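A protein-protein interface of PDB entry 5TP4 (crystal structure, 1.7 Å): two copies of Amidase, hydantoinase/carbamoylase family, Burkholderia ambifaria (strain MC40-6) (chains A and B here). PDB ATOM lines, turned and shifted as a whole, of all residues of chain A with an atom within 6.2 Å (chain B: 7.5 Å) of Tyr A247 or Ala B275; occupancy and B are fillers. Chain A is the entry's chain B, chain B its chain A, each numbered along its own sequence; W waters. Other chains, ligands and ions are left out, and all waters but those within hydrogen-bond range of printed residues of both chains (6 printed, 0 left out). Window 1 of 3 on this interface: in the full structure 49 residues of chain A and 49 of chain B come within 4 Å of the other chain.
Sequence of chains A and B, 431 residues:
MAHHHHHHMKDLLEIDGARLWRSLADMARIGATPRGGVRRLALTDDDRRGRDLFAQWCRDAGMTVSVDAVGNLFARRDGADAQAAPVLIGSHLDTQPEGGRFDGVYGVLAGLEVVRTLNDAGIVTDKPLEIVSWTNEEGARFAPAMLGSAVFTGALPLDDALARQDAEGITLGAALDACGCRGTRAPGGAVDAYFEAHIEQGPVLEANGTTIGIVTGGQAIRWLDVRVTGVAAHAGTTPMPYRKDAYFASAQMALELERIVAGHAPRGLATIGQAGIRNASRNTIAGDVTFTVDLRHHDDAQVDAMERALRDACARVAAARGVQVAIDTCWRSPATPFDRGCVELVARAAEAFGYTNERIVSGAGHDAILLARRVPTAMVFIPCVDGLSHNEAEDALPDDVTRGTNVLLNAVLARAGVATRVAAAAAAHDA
The backbone carbonyl oxygen (O) of Ala B275 is in hydrogen-bond range of the backbone NH (N) of Ile A277.
The backbone NH of Ile B277 lies within hydrogen-bond range of the backbone carbonyl oxygen of Ala A275 (3.3 Å).
The backbone carbonyl oxygen of Gln B274 is in hydrogen-bond range of the backbone NH of Thr B292 (2.9 Å).
The backbone NH (N) of Gly B276 lies within hydrogen-bond range of the backbone carbonyl oxygen (O) of Thr B290, at 2.9 Å.
N of Phe A248 lies within hydrogen-bond range of OD1 of Asp A245.
The backbone NH (N) of Tyr A247 lies within hydrogen-bond range of the side-chain carboxylate (OD1) of Asp A245 (2.8 Å).
Among the printed residues, merely in contact across the chains: Tyr A247 with Ala B254 (3.98 Å), Tyr A247 with Ile B272 (3.5 Å), Tyr A247 with Ala B275 (3.6 Å), Phe A248 with Ala B254 (3.2 Å), Phe A248 with Leu B255 (3.8 Å), Ala A251 with Ala B251 (3.7 Å), Ala A251 with Ala B254 (3.9 Å), Gln A252 with Leu B255 (3.8 Å), Ala A275 with Tyr B247 (3.7 Å), Ala A275 with Gly B276 (3.2 Å), Gly A276 with Ala B275 (3.3 Å), Ile A277 with Ile B272 (3.3 Å), Ile A277 with Gly B273 (3.4 Å), Ile A277 with Gln B274 (3.7 Å), Ala A280 with Gly B273 (3.2 Å) and Ala A280 with Gln B274 (3.8 Å).
Of the printed residues of chain B, Tyr A247 touches Ala B254 (3.98 Å), Ile B272 (3.5 Å) and Ala B275 (3.6 Å).
Of the printed residues of chain A, Ala B275 touches Tyr A247 (3.6 Å), Gly A276 (3.3 Å) and Ile A277 (3.3 Å).
Ala A246 touches none of the printed residues of chain B.
Of the printed residues of chain B, Gly A276 touches Ala B275.
Of the printed residues of chain B, Gln A252 touches Leu B255 (3.8 Å).
Of the printed residues of chain B, Phe A248 touches Ala B254 (3.2 Å) and Leu B255 (3.8 Å).
Of the printed residues of chain B, Ala A280 touches Gly B273 (3.2 Å) and Gln B274 (3.8 Å).
Printed residues of chain A within 4 Å of Tyr B247: Ala A275 (3.7 Å).
Val A228 touches none of the printed residues of chain B.
Arg B278 touches none of the printed residues of chain A.
Hydrophobic or aromatic side chains of chain A within 4 Å of the printed part of chain B: Tyr A247, Phe A248, Ala A251, Ala A275, Ile A277 and Ala A280.
Of the 19 printed residues of chain B, 10 touch a printed residue of chain A.
Hydrophobic or aromatic side chains of chain B within 4 Å of the printed part of chain A: Tyr B247, Ala B251, Ala B254, Leu B255, Ile B272, Ala B275 and Ile B277.
Among the printed residues, no Asp or Glu carboxylate lies within 4 Å of a Lys or Arg side-chain nitrogen of the other chain.
Tyr A247 touches Ala B275, and with the chains exchanged Ala A275 touches Tyr B247.
Ala B251 touches its own counterpart, Ala A251.
Ala A275 touches Gly B276, and with the chains exchanged Gly A276 touches Ala B275.
Ala A275 touches Ile B277, and with the chains exchanged Ile A277 touches Ala B275.
8 positions are printed for both chains.
Of the 18 pairs that touch across the chains among the printed residues, 7 have their exchanged pair printed and touching as well.
Water W3 bridges the backbone carbonyl oxygen (O) of Ser A250 and the side-chain hydroxyl (OH) of Tyr B247.
Water W2 bridges the backbone NH of Ile B272 (2.7 Å) and the side-chain carboxylate of Asp A245 (2.7 Å).
Water W4 lies within hydrogen-bond range of N of Ala A286, O of Ile B272 and OD2 of Asp A245.
Water W6 lies within hydrogen-bond range of the side-chain hydroxyl of Tyr A247 (2.8 Å) and the backbone carbonyl oxygen of Ser B250 (2.8 Å).
Water W5 lies within hydrogen-bond range of the backbone NH of Ala A275 and the backbone carbonyl oxygen of Ile B277.
Water W1 bridges O of Ile A277 and N of Ala B275.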
ATOM      1  N   VAL A 228      -2.033  -2.794  -5.114  1.00  0.00           N
ATOM      2  CA  VAL A 228      -2.755  -2.506  -6.348  1.00  0.00           C
ATOM      3  C   VAL A 228      -4.016  -1.736  -5.984  1.00  0.00           C
ATOM      4  O   VAL A 228      -4.769  -2.157  -5.099  1.00  0.00           O
ATOM      5  CB  VAL A 228      -3.106  -3.800  -7.107  1.00  0.00           C
ATOM      6  CG1 VAL A 228      -3.730  -3.469  -8.449  1.00  0.00           C
ATOM      7  CG2 VAL A 228      -1.849  -4.656  -7.290  1.00  0.00           C
ATOM      8  N   LYS A 244     -12.590  -1.374 -12.576  1.00  0.00           N
ATOM      9  CA  LYS A 244     -11.144  -1.261 -12.373  1.00  0.00           C
ATOM     10  C   LYS A 244     -10.839  -2.168 -11.173  1.00  0.00           C
ATOM     11  O   LYS A 244     -10.688  -1.725 -10.036  1.00  0.00           O
ATOM     12  CB  LYS A 244     -10.742   0.173 -12.164  1.00  0.00           C
ATOM     13  CG  LYS A 244     -10.977   1.017 -13.444  1.00  0.00           C
ATOM     14  CD  LYS A 244     -10.856   2.492 -13.154  1.00  0.00           C
ATOM     15  CE  LYS A 244     -11.347   3.337 -14.322  1.00  0.00           C
ATOM     16  NZ  LYS A 244     -11.175   4.800 -14.033  1.00  0.00           N
ATOM     17  N   ASP A 245     -10.788  -3.471 -11.453  1.00  0.00           N
ATOM     18  CA  ASP A 245     -10.797  -4.509 -10.434  1.00  0.00           C
ATOM     19  C   ASP A 245      -9.363  -4.809 -10.017  1.00  0.00           C
ATOM     20  O   ASP A 245      -8.616  -5.435 -10.774  1.00  0.00           O
ATOM     21  CB  ASP A 245     -11.486  -5.754 -10.995  1.00  0.00           C
ATOM     22  CG  ASP A 245     -11.693  -6.835  -9.952  1.00  0.00           C
ATOM     23  OD1 ASP A 245     -10.775  -7.085  -9.155  1.00  0.00           O
ATOM     24  OD2 ASP A 245     -12.762  -7.482  -9.957  1.00  0.00           O
ATOM     25  N   ALA A 246      -8.987  -4.370  -8.811  1.00  0.00           N
ATOM     26  CA  ALA A 246      -7.629  -4.570  -8.330  1.00  0.00           C
ATOM     27  C   ALA A 246      -7.315  -6.034  -8.055  1.00  0.00           C
ATOM     28  O   ALA A 246      -6.127  -6.390  -7.997  1.00  0.00           O
ATOM     29  CB  ALA A 246      -7.379  -3.738  -7.066  1.00  0.00           C
ATOM     30  N   TYR A 247      -8.331  -6.887  -7.856  1.00  0.00           N
ATOM     31  CA  TYR A 247      -7.997  -8.274  -7.558  1.00  0.00           C
ATOM     32  C   TYR A 247      -7.747  -9.068  -8.828  1.00  0.00           C
ATOM     33  O   TYR A 247      -6.798  -9.859  -8.874  1.00  0.00           O
ATOM     34  CB  TYR A 247      -9.078  -8.944  -6.705  1.00  0.00           C
ATOM     35  CG  TYR A 247      -8.639 -10.350  -6.356  1.00  0.00           C
ATOM     36  CD1 TYR A 247      -7.658 -10.573  -5.379  1.00  0.00           C
ATOM     37  CD2 TYR A 247      -9.145 -11.440  -7.047  1.00  0.00           C
ATOM     38  CE1 TYR A 247      -7.230 -11.867  -5.077  1.00  0.00           C
ATOM     39  CE2 TYR A 247      -8.724 -12.746  -6.748  1.00  0.00           C
ATOM     40  CZ  TYR A 247      -7.772 -12.939  -5.780  1.00  0.00           C
ATOM     41  OH  TYR A 247      -7.363 -14.218  -5.486  1.00  0.00           O
ATOM     42  N   PHE A 248      -8.551  -8.861  -9.878  1.00  0.00           N
ATOM     43  CA  PHE A 248      -8.223  -9.517 -11.144  1.00  0.00           C
ATOM     44  C   PHE A 248      -6.877  -9.025 -11.646  1.00  0.00           C
ATOM     45  O   PHE A 248      -6.121  -9.800 -12.241  1.00  0.00           O
ATOM     46  CB  PHE A 248      -9.283  -9.261 -12.233  1.00  0.00           C
ATOM     47  CG  PHE A 248     -10.511 -10.148 -12.155  1.00  0.00           C
ATOM     48  CD1 PHE A 248     -10.460 -11.426 -11.617  1.00  0.00           C
ATOM     49  CD2 PHE A 248     -11.728  -9.682 -12.660  1.00  0.00           C
ATOM     50  CE1 PHE A 248     -11.625 -12.231 -11.572  1.00  0.00           C
ATOM     51  CE2 PHE A 248     -12.885 -10.470 -12.605  1.00  0.00           C
ATOM     52  CZ  PHE A 248     -12.822 -11.740 -12.059  1.00  0.00           C
ATOM     53  N   ALA A 249      -6.565  -7.747 -11.409  1.00  0.00           N
ATOM     54  CA  ALA A 249      -5.257  -7.218 -11.799  1.00  0.00           C
ATOM     55  C   ALA A 249      -4.139  -7.908 -11.026  1.00  0.00           C
ATOM     56  O   ALA A 249      -3.118  -8.310 -11.605  1.00  0.00           O
ATOM     57  CB  ALA A 249      -5.205  -5.705 -11.574  1.00  0.00           C
ATOM     58  N   SER A 250      -4.324  -8.066  -9.715  1.00  0.00           N
ATOM     59  CA  SER A 250      -3.318  -8.719  -8.891  1.00  0.00           C
ATOM     60  C   SER A 250      -3.117 -10.153  -9.310  1.00  0.00           C
ATOM     61  O   SER A 250      -2.011 -10.696  -9.200  1.00  0.00           O
ATOM     62  CB  SER A 250      -3.722  -8.675  -7.416  1.00  0.00           C
ATOM     63  OG  SER A 250      -3.677  -7.346  -6.913  1.00  0.00           O
ATOM     64  N   ALA A 251      -4.207 -10.824  -9.692  1.00  0.00           N
ATOM     65  CA  ALA A 251      -4.097 -12.197 -10.145  1.00  0.00           C
ATOM     66  C   ALA A 251      -3.278 -12.287 -11.422  1.00  0.00           C
ATOM     67  O   ALA A 251      -2.424 -13.171 -11.552  1.00  0.00           O
ATOM     68  CB  ALA A 251      -5.498 -12.792 -10.345  1.00  0.00           C
ATOM     69  N   GLN A 252      -3.493 -11.363 -12.367  1.00  0.00           N
ATOM     70  CA  GLN A 252      -2.675 -11.408 -13.576  1.00  0.00           C
ATOM     71  C   GLN A 252      -1.219 -11.119 -13.256  1.00  0.00           C
ATOM     72  O   GLN A 252      -0.310 -11.716 -13.858  1.00  0.00           O
ATOM     73  CB  GLN A 252      -3.180 -10.435 -14.636  1.00  0.00           C
ATOM     74  CG  GLN A 252      -2.396 -10.644 -15.917  1.00  0.00           C
ATOM     75  CD  GLN A 252      -2.890  -9.816 -17.046  1.00  0.00           C
ATOM     76  OE1 GLN A 252      -3.768  -8.980 -16.872  1.00  0.00           O
ATOM     77  NE2 GLN A 252      -2.324 -10.033 -18.230  1.00  0.00           N
ATOM     78  N   ALA A 275      -1.316 -12.185   1.152  1.00  0.00           N
ATOM     79  CA  ALA A 275      -2.117 -11.454   0.185  1.00  0.00           C
ATOM     80  C   ALA A 275      -3.511 -11.261   0.744  1.00  0.00           C
ATOM     81  O   ALA A 275      -4.040 -12.140   1.449  1.00  0.00           O
ATOM     82  CB  ALA A 275      -2.178 -12.179  -1.171  1.00  0.00           C
ATOM     83  N   GLY A 276      -4.103 -10.110   0.441  1.00  0.00           N
ATOM     84  CA  GLY A 276      -5.453  -9.857   0.910  1.00  0.00           C
ATOM     85  C   GLY A 276      -6.099  -8.696   0.193  1.00  0.00           C
ATOM     86  O   GLY A 276      -5.429  -7.749  -0.236  1.00  0.00           O
ATOM     87  N   ILE A 277      -7.416  -8.765   0.085  1.00  0.00           N
ATOM     88  CA  ILE A 277      -8.228  -7.633  -0.336  1.00  0.00           C
ATOM     89  C   ILE A 277      -8.576  -6.856   0.917  1.00  0.00           C
ATOM     90  O   ILE A 277      -9.156  -7.420   1.852  1.00  0.00           O
ATOM     91  CB  ILE A 277      -9.498  -8.109  -1.059  1.00  0.00           C
ATOM     92  CG1 ILE A 277      -9.131  -8.902  -2.318  1.00  0.00           C
ATOM     93  CG2 ILE A 277     -10.392  -6.911  -1.405  1.00  0.00           C
ATOM     94  CD1 ILE A 277     -10.331  -9.576  -2.970  1.00  0.00           C
ATOM     95  N   ALA A 280     -12.720  -5.354   2.680  1.00  0.00           N
ATOM     96  CA  ALA A 280     -13.330  -6.246   1.695  1.00  0.00           C
ATOM     97  C   ALA A 280     -14.773  -6.594   2.053  1.00  0.00           C
ATOM     98  O   ALA A 280     -15.120  -6.729   3.228  1.00  0.00           O
ATOM     99  CB  ALA A 280     -12.505  -7.530   1.607  1.00  0.00           C
ATOM    100  N   ALA A 286     -12.907  -5.283  -5.588  1.00  0.00           N
ATOM    101  CA  ALA A 286     -11.679  -4.953  -4.865  1.00  0.00           C
ATOM    102  C   ALA A 286     -11.086  -3.653  -5.397  1.00  0.00           C
ATOM    103  O   ALA A 286     -10.801  -3.539  -6.593  1.00  0.00           O
ATOM    104  CB  ALA A 286     -10.667  -6.092  -4.996  1.00  0.00           C
ATOM    105  N   GLY A 287     -10.919  -2.673  -4.509  1.00  0.00           N
ATOM    106  CA  GLY A 287     -10.246  -1.436  -4.862  1.00  0.00           C
ATOM    107  C   GLY A 287      -8.852  -1.326  -4.270  1.00  0.00           C
ATOM    108  O   GLY A 287      -8.126  -0.382  -4.593  1.00  0.00           O
ATOM    109  N   VAL A 289      -5.701  -3.964  -2.954  1.00  0.00           N
ATOM    110  CA  VAL A 289      -5.183  -5.317  -2.779  1.00  0.00           C
ATOM    111  C   VAL A 289      -3.707  -5.204  -2.453  1.00  0.00           C
ATOM    112  O   VAL A 289      -2.981  -4.453  -3.117  1.00  0.00           O
ATOM    113  CB  VAL A 289      -5.363  -6.180  -4.038  1.00  0.00           C
ATOM    114  CG1 VAL A 289      -4.768  -7.570  -3.794  1.00  0.00           C
ATOM    115  CG2 VAL A 289      -6.858  -6.283  -4.431  1.00  0.00           C
ATOM    116  N   TYR B 247      -1.708 -20.181  -3.965  1.00  0.00           N
ATOM    117  CA  TYR B 247      -2.002 -18.814  -4.369  1.00  0.00           C
ATOM    118  C   TYR B 247      -1.852 -18.638  -5.879  1.00  0.00           C
ATOM    119  O   TYR B 247      -2.711 -18.032  -6.530  1.00  0.00           O
ATOM    120  CB  TYR B 247      -1.119 -17.809  -3.612  1.00  0.00           C
ATOM    121  CG  TYR B 247      -1.529 -16.408  -3.994  1.00  0.00           C
ATOM    122  CD1 TYR B 247      -2.694 -15.853  -3.472  1.00  0.00           C
ATOM    123  CD2 TYR B 247      -0.822 -15.696  -4.960  1.00  0.00           C
ATOM    124  CE1 TYR B 247      -3.107 -14.585  -3.864  1.00  0.00           C
ATOM    125  CE2 TYR B 247      -1.236 -14.437  -5.359  1.00  0.00           C
ATOM    126  CZ  TYR B 247      -2.377 -13.895  -4.803  1.00  0.00           C
ATOM    127  OH  TYR B 247      -2.791 -12.639  -5.178  1.00  0.00           O
ATOM    128  N   SER B 250      -4.947 -20.095  -7.147  1.00  0.00           N
ATOM    129  CA  SER B 250      -6.113 -19.231  -7.003  1.00  0.00           C
ATOM    130  C   SER B 250      -6.065 -18.085  -8.010  1.00  0.00           C
ATOM    131  O   SER B 250      -7.098 -17.652  -8.531  1.00  0.00           O
ATOM    132  CB  SER B 250      -6.192 -18.679  -5.586  1.00  0.00           C
ATOM    133  OG  SER B 250      -6.396 -19.693  -4.623  1.00  0.00           O
ATOM    134  N   ALA B 251      -4.866 -17.553  -8.278  1.00  0.00           N
ATOM    135  CA  ALA B 251      -4.754 -16.501  -9.282  1.00  0.00           C
ATOM    136  C   ALA B 251      -5.191 -17.008 -10.652  1.00  0.00           C
ATOM    137  O   ALA B 251      -5.935 -16.331 -11.378  1.00  0.00           O
ATOM    138  CB  ALA B 251      -3.310 -15.969  -9.324  1.00  0.00           C
ATOM    139  N   GLN B 252      -4.794 -18.228 -11.007  1.00  0.00           N
ATOM    140  CA  GLN B 252      -5.225 -18.736 -12.301  1.00  0.00           C
ATOM    141  C   GLN B 252      -6.726 -18.971 -12.317  1.00  0.00           C
ATOM    142  O   GLN B 252      -7.385 -18.737 -13.341  1.00  0.00           O
ATOM    143  CB  GLN B 252      -4.479 -20.015 -12.672  1.00  0.00           C
ATOM    144  CG  GLN B 252      -4.863 -20.419 -14.089  1.00  0.00           C
ATOM    145  CD  GLN B 252      -4.127 -21.609 -14.618  1.00  0.00           C
ATOM    146  OE1 GLN B 252      -3.322 -22.231 -13.920  1.00  0.00           O
ATOM    147  NE2 GLN B 252      -4.403 -21.949 -15.874  1.00  0.00           N
ATOM    148  N   MET B 253      -7.287 -19.431 -11.196  1.00  0.00           N
ATOM    149  CA  MET B 253      -8.738 -19.614 -11.161  1.00  0.00           C
ATOM    150  C   MET B 253      -9.449 -18.285 -11.364  1.00  0.00           C
ATOM    151  O   MET B 253     -10.492 -18.221 -12.024  1.00  0.00           O
ATOM    152  CB  MET B 253      -9.152 -20.243  -9.841  1.00  0.00           C
ATOM    153  CG  MET B 253      -8.640 -21.662  -9.700  1.00  0.00           C
ATOM    154  SD  MET B 253      -8.989 -22.353  -8.069  1.00  0.00           S
ATOM    155  CE  MET B 253      -7.972 -23.837  -8.116  1.00  0.00           C
ATOM    156  N   ALA B 254      -8.890 -17.211 -10.814  1.00  0.00           N
ATOM    157  CA  ALA B 254      -9.521 -15.905 -10.964  1.00  0.00           C
ATOM    158  C   ALA B 254      -9.556 -15.496 -12.422  1.00  0.00           C
ATOM    159  O   ALA B 254     -10.542 -14.923 -12.900  1.00  0.00           O
ATOM    160  CB  ALA B 254      -8.769 -14.858 -10.123  1.00  0.00           C
ATOM    161  N   LEU B 255      -8.497 -15.799 -13.156  1.00  0.00           N
ATOM    162  CA  LEU B 255      -8.484 -15.426 -14.558  1.00  0.00           C
ATOM    163  C   LEU B 255      -9.378 -16.352 -15.380  1.00  0.00           C
ATOM    164  O   LEU B 255      -9.973 -15.909 -16.372  1.00  0.00           O
ATOM    165  CB  LEU B 255      -7.033 -15.393 -15.055  1.00  0.00           C
ATOM    166  CG  LEU B 255      -6.137 -14.386 -14.284  1.00  0.00           C
ATOM    167  CD1 LEU B 255      -4.773 -14.272 -14.933  1.00  0.00           C
ATOM    168  CD2 LEU B 255      -6.751 -12.976 -14.161  1.00  0.00           C
ATOM    169  N   THR B 271     -17.382 -11.187  -9.419  1.00  0.00           N
ATOM    170  CA  THR B 271     -16.550 -10.367  -8.551  1.00  0.00           C
ATOM    171  C   THR B 271     -15.942 -11.243  -7.475  1.00  0.00           C
ATOM    172  O   THR B 271     -16.667 -11.992  -6.810  1.00  0.00           O
ATOM    173  CB  THR B 271     -17.394  -9.269  -7.886  1.00  0.00           C
ATOM    174  OG1 THR B 271     -18.214  -8.619  -8.870  1.00  0.00           O
ATOM    175  CG2 THR B 271     -16.503  -8.256  -7.248  1.00  0.00           C
ATOM    176  N   ILE B 272     -14.632 -11.092  -7.241  1.00  0.00           N
ATOM    177  CA  ILE B 272     -13.971 -11.709  -6.092  1.00  0.00           C
ATOM    178  C   ILE B 272     -13.732 -10.590  -5.088  1.00  0.00           C
ATOM    179  O   ILE B 272     -12.791  -9.803  -5.228  1.00  0.00           O
ATOM    180  CB  ILE B 272     -12.685 -12.434  -6.506  1.00  0.00           C
ATOM    181  CG1 ILE B 272     -13.060 -13.651  -7.391  1.00  0.00           C
ATOM    182  CG2 ILE B 272     -11.897 -12.897  -5.279  1.00  0.00           C
ATOM    183  CD1 ILE B 272     -11.852 -14.339  -8.086  1.00  0.00           C
ATOM    184  N   GLY B 273     -14.608 -10.483  -4.085  1.00  0.00           N
ATOM    185  CA  GLY B 273     -14.517  -9.332  -3.195  1.00  0.00           C
ATOM    186  C   GLY B 273     -13.719  -9.557  -1.925  1.00  0.00           C
ATOM    187  O   GLY B 273     -13.303  -8.588  -1.277  1.00  0.00           O
ATOM    188  N   GLN B 274     -13.515 -10.823  -1.546  1.00  0.00           N
ATOM    189  CA  GLN B 274     -12.732 -11.185  -0.375  1.00  0.00           C
ATOM    190  C   GLN B 274     -11.764 -12.267  -0.810  1.00  0.00           C
ATOM    191  O   GLN B 274     -12.132 -13.157  -1.592  1.00  0.00           O
ATOM    192  CB  GLN B 274     -13.603 -11.690   0.789  1.00  0.00           C
ATOM    193  CG  GLN B 274     -14.664 -10.692   1.290  1.00  0.00           C
ATOM    194  CD  GLN B 274     -15.488 -11.245   2.429  1.00  0.00           C
ATOM    195  OE1 GLN B 274     -15.591 -12.457   2.600  1.00  0.00           O
ATOM    196  NE2 GLN B 274     -16.066 -10.360   3.229  1.00  0.00           N
ATOM    197  N   ALA B 275     -10.535 -12.179  -0.319  1.00  0.00           N
ATOM    198  CA  ALA B 275      -9.528 -13.169  -0.681  1.00  0.00           C
ATOM    199  C   ALA B 275      -8.380 -13.039   0.292  1.00  0.00           C
ATOM    200  O   ALA B 275      -8.015 -11.920   0.684  1.00  0.00           O
ATOM    201  CB  ALA B 275      -9.055 -12.976  -2.126  1.00  0.00           C
ATOM    202  N   GLY B 276      -7.825 -14.171   0.702  1.00  0.00           N
ATOM    203  CA  GLY B 276      -6.621 -14.104   1.509  1.00  0.00           C
ATOM    204  C   GLY B 276      -5.928 -15.441   1.633  1.00  0.00           C
ATOM    205  O   GLY B 276      -6.545 -16.506   1.516  1.00  0.00           O
ATOM    206  N   ILE B 277      -4.629 -15.364   1.903  1.00  0.00           N
ATOM    207  CA  ILE B 277      -3.818 -16.520   2.279  1.00  0.00           C
ATOM    208  C   ILE B 277      -3.912 -16.674   3.787  1.00  0.00           C
ATOM    209  O   ILE B 277      -3.643 -15.723   4.529  1.00  0.00           O
ATOM    210  CB  ILE B 277      -2.355 -16.330   1.835  1.00  0.00           C
ATOM    211  CG1 ILE B 277      -2.297 -16.110   0.325  1.00  0.00           C
ATOM    212  CG2 ILE B 277      -1.494 -17.518   2.287  1.00  0.00           C
ATOM    213  CD1 ILE B 277      -0.913 -15.745  -0.200  1.00  0.00           C
ATOM    214  N   ARG B 278      -4.309 -17.857   4.251  1.00  0.00           N
ATOM    215  CA  ARG B 278      -4.463 -18.086   5.679  1.00  0.00           C
ATOM    216  C   ARG B 278      -3.158 -18.581   6.290  1.00  0.00           C
ATOM    217  O   ARG B 278      -2.357 -19.258   5.633  1.00  0.00           O
ATOM    218  CB  ARG B 278      -5.589 -19.088   5.948  1.00  0.00           C
ATOM    219  CG  ARG B 278      -6.973 -18.622   5.432  1.00  0.00           C
ATOM    220  CD  ARG B 278      -8.072 -19.650   5.731  1.00  0.00           C
ATOM    221  NE  ARG B 278      -8.528 -19.600   7.119  1.00  0.00           N
ATOM    222  CZ  ARG B 278      -8.114 -20.423   8.079  1.00  0.00           C
ATOM    223  NH1 ARG B 278      -7.230 -21.375   7.811  1.00  0.00           N
ATOM    224  NH2 ARG B 278      -8.586 -20.300   9.312  1.00  0.00           N
ATOM    225  N   VAL B 289      -5.752 -21.060   0.784  1.00  0.00           N
ATOM    226  CA  VAL B 289      -6.213 -19.785   0.242  1.00  0.00           C
ATOM    227  C   VAL B 289      -7.731 -19.840   0.170  1.00  0.00           C
ATOM    228  O   VAL B 289      -8.294 -20.828  -0.317  1.00  0.00           O
ATOM    229  CB  VAL B 289      -5.618 -19.509  -1.155  1.00  0.00           C
ATOM    230  CG1 VAL B 289      -6.201 -18.222  -1.788  1.00  0.00           C
ATOM    231  CG2 VAL B 289      -4.081 -19.411  -1.071  1.00  0.00           C
ATOM    232  N   THR B 290      -8.396 -18.797   0.650  1.00  0.00           N
ATOM    233  CA  THR B 290      -9.842 -18.692   0.508  1.00  0.00           C
ATOM    234  C   THR B 290     -10.175 -17.444  -0.282  1.00  0.00           C
ATOM    235  O   THR B 290      -9.487 -16.425  -0.181  1.00  0.00           O
ATOM    236  CB  THR B 290     -10.584 -18.629   1.862  1.00  0.00           C
ATOM    237  OG1 THR B 290     -10.110 -17.510   2.627  1.00  0.00           O
ATOM    238  CG2 THR B 290     -10.421 -19.937   2.674  1.00  0.00           C
ATOM    239  N   PHE B 291     -11.223 -17.515  -1.089  1.00  0.00           N
ATOM    240  CA  PHE B 291     -11.733 -16.291  -1.685  1.00  0.00           C
ATOM    241  C   PHE B 291     -13.217 -16.477  -1.916  1.00  0.00           C
ATOM    242  O   PHE B 291     -13.721 -17.599  -1.896  1.00  0.00           O
ATOM    243  CB  PHE B 291     -10.981 -15.925  -2.979  1.00  0.00           C
ATOM    244  CG  PHE B 291     -11.022 -16.977  -4.077  1.00  0.00           C
ATOM    245  CD1 PHE B 291     -10.067 -17.979  -4.151  1.00  0.00           C
ATOM    246  CD2 PHE B 291     -11.957 -16.880  -5.103  1.00  0.00           C
ATOM    247  CE1 PHE B 291     -10.064 -18.895  -5.204  1.00  0.00           C
ATOM    248  CE2 PHE B 291     -11.959 -17.795  -6.168  1.00  0.00           C
ATOM    249  CZ  PHE B 291     -11.004 -18.803  -6.221  1.00  0.00           C
ATOM    250  N   THR B 292     -13.924 -15.368  -2.100  1.00  0.00           N
ATOM    251  CA  THR B 292     -15.358 -15.436  -2.346  1.00  0.00           C
ATOM    252  C   THR B 292     -15.630 -15.057  -3.794  1.00  0.00           C
ATOM    253  O   THR B 292     -14.849 -14.336  -4.425  1.00  0.00           O
ATOM    254  CB  THR B 292     -16.143 -14.496  -1.414  1.00  0.00           C
ATOM    255  OG1 THR B 292     -15.772 -13.133  -1.667  1.00  0.00           O
ATOM    256  CG2 THR B 292     -15.929 -14.857   0.046  1.00  0.00           C
HETATM  257  O   HOH W   1     -10.377 -10.047   1.897  1.00  0.00           O
HETATM  258  O   HOH W   2     -12.896 -10.091  -9.109  1.00  0.00           O
HETATM  259  O   HOH W   3      -0.993 -11.250  -6.747  1.00  0.00           O
HETATM  260  O   HOH W   4     -12.980  -7.661  -6.989  1.00  0.00           O
HETATM  261  O   HOH W   5      -2.225 -13.156   3.679  1.00  0.00           O
HETATM  262  O   HOH W   6      -8.816 -16.192  -6.834  1.00  0.00           O
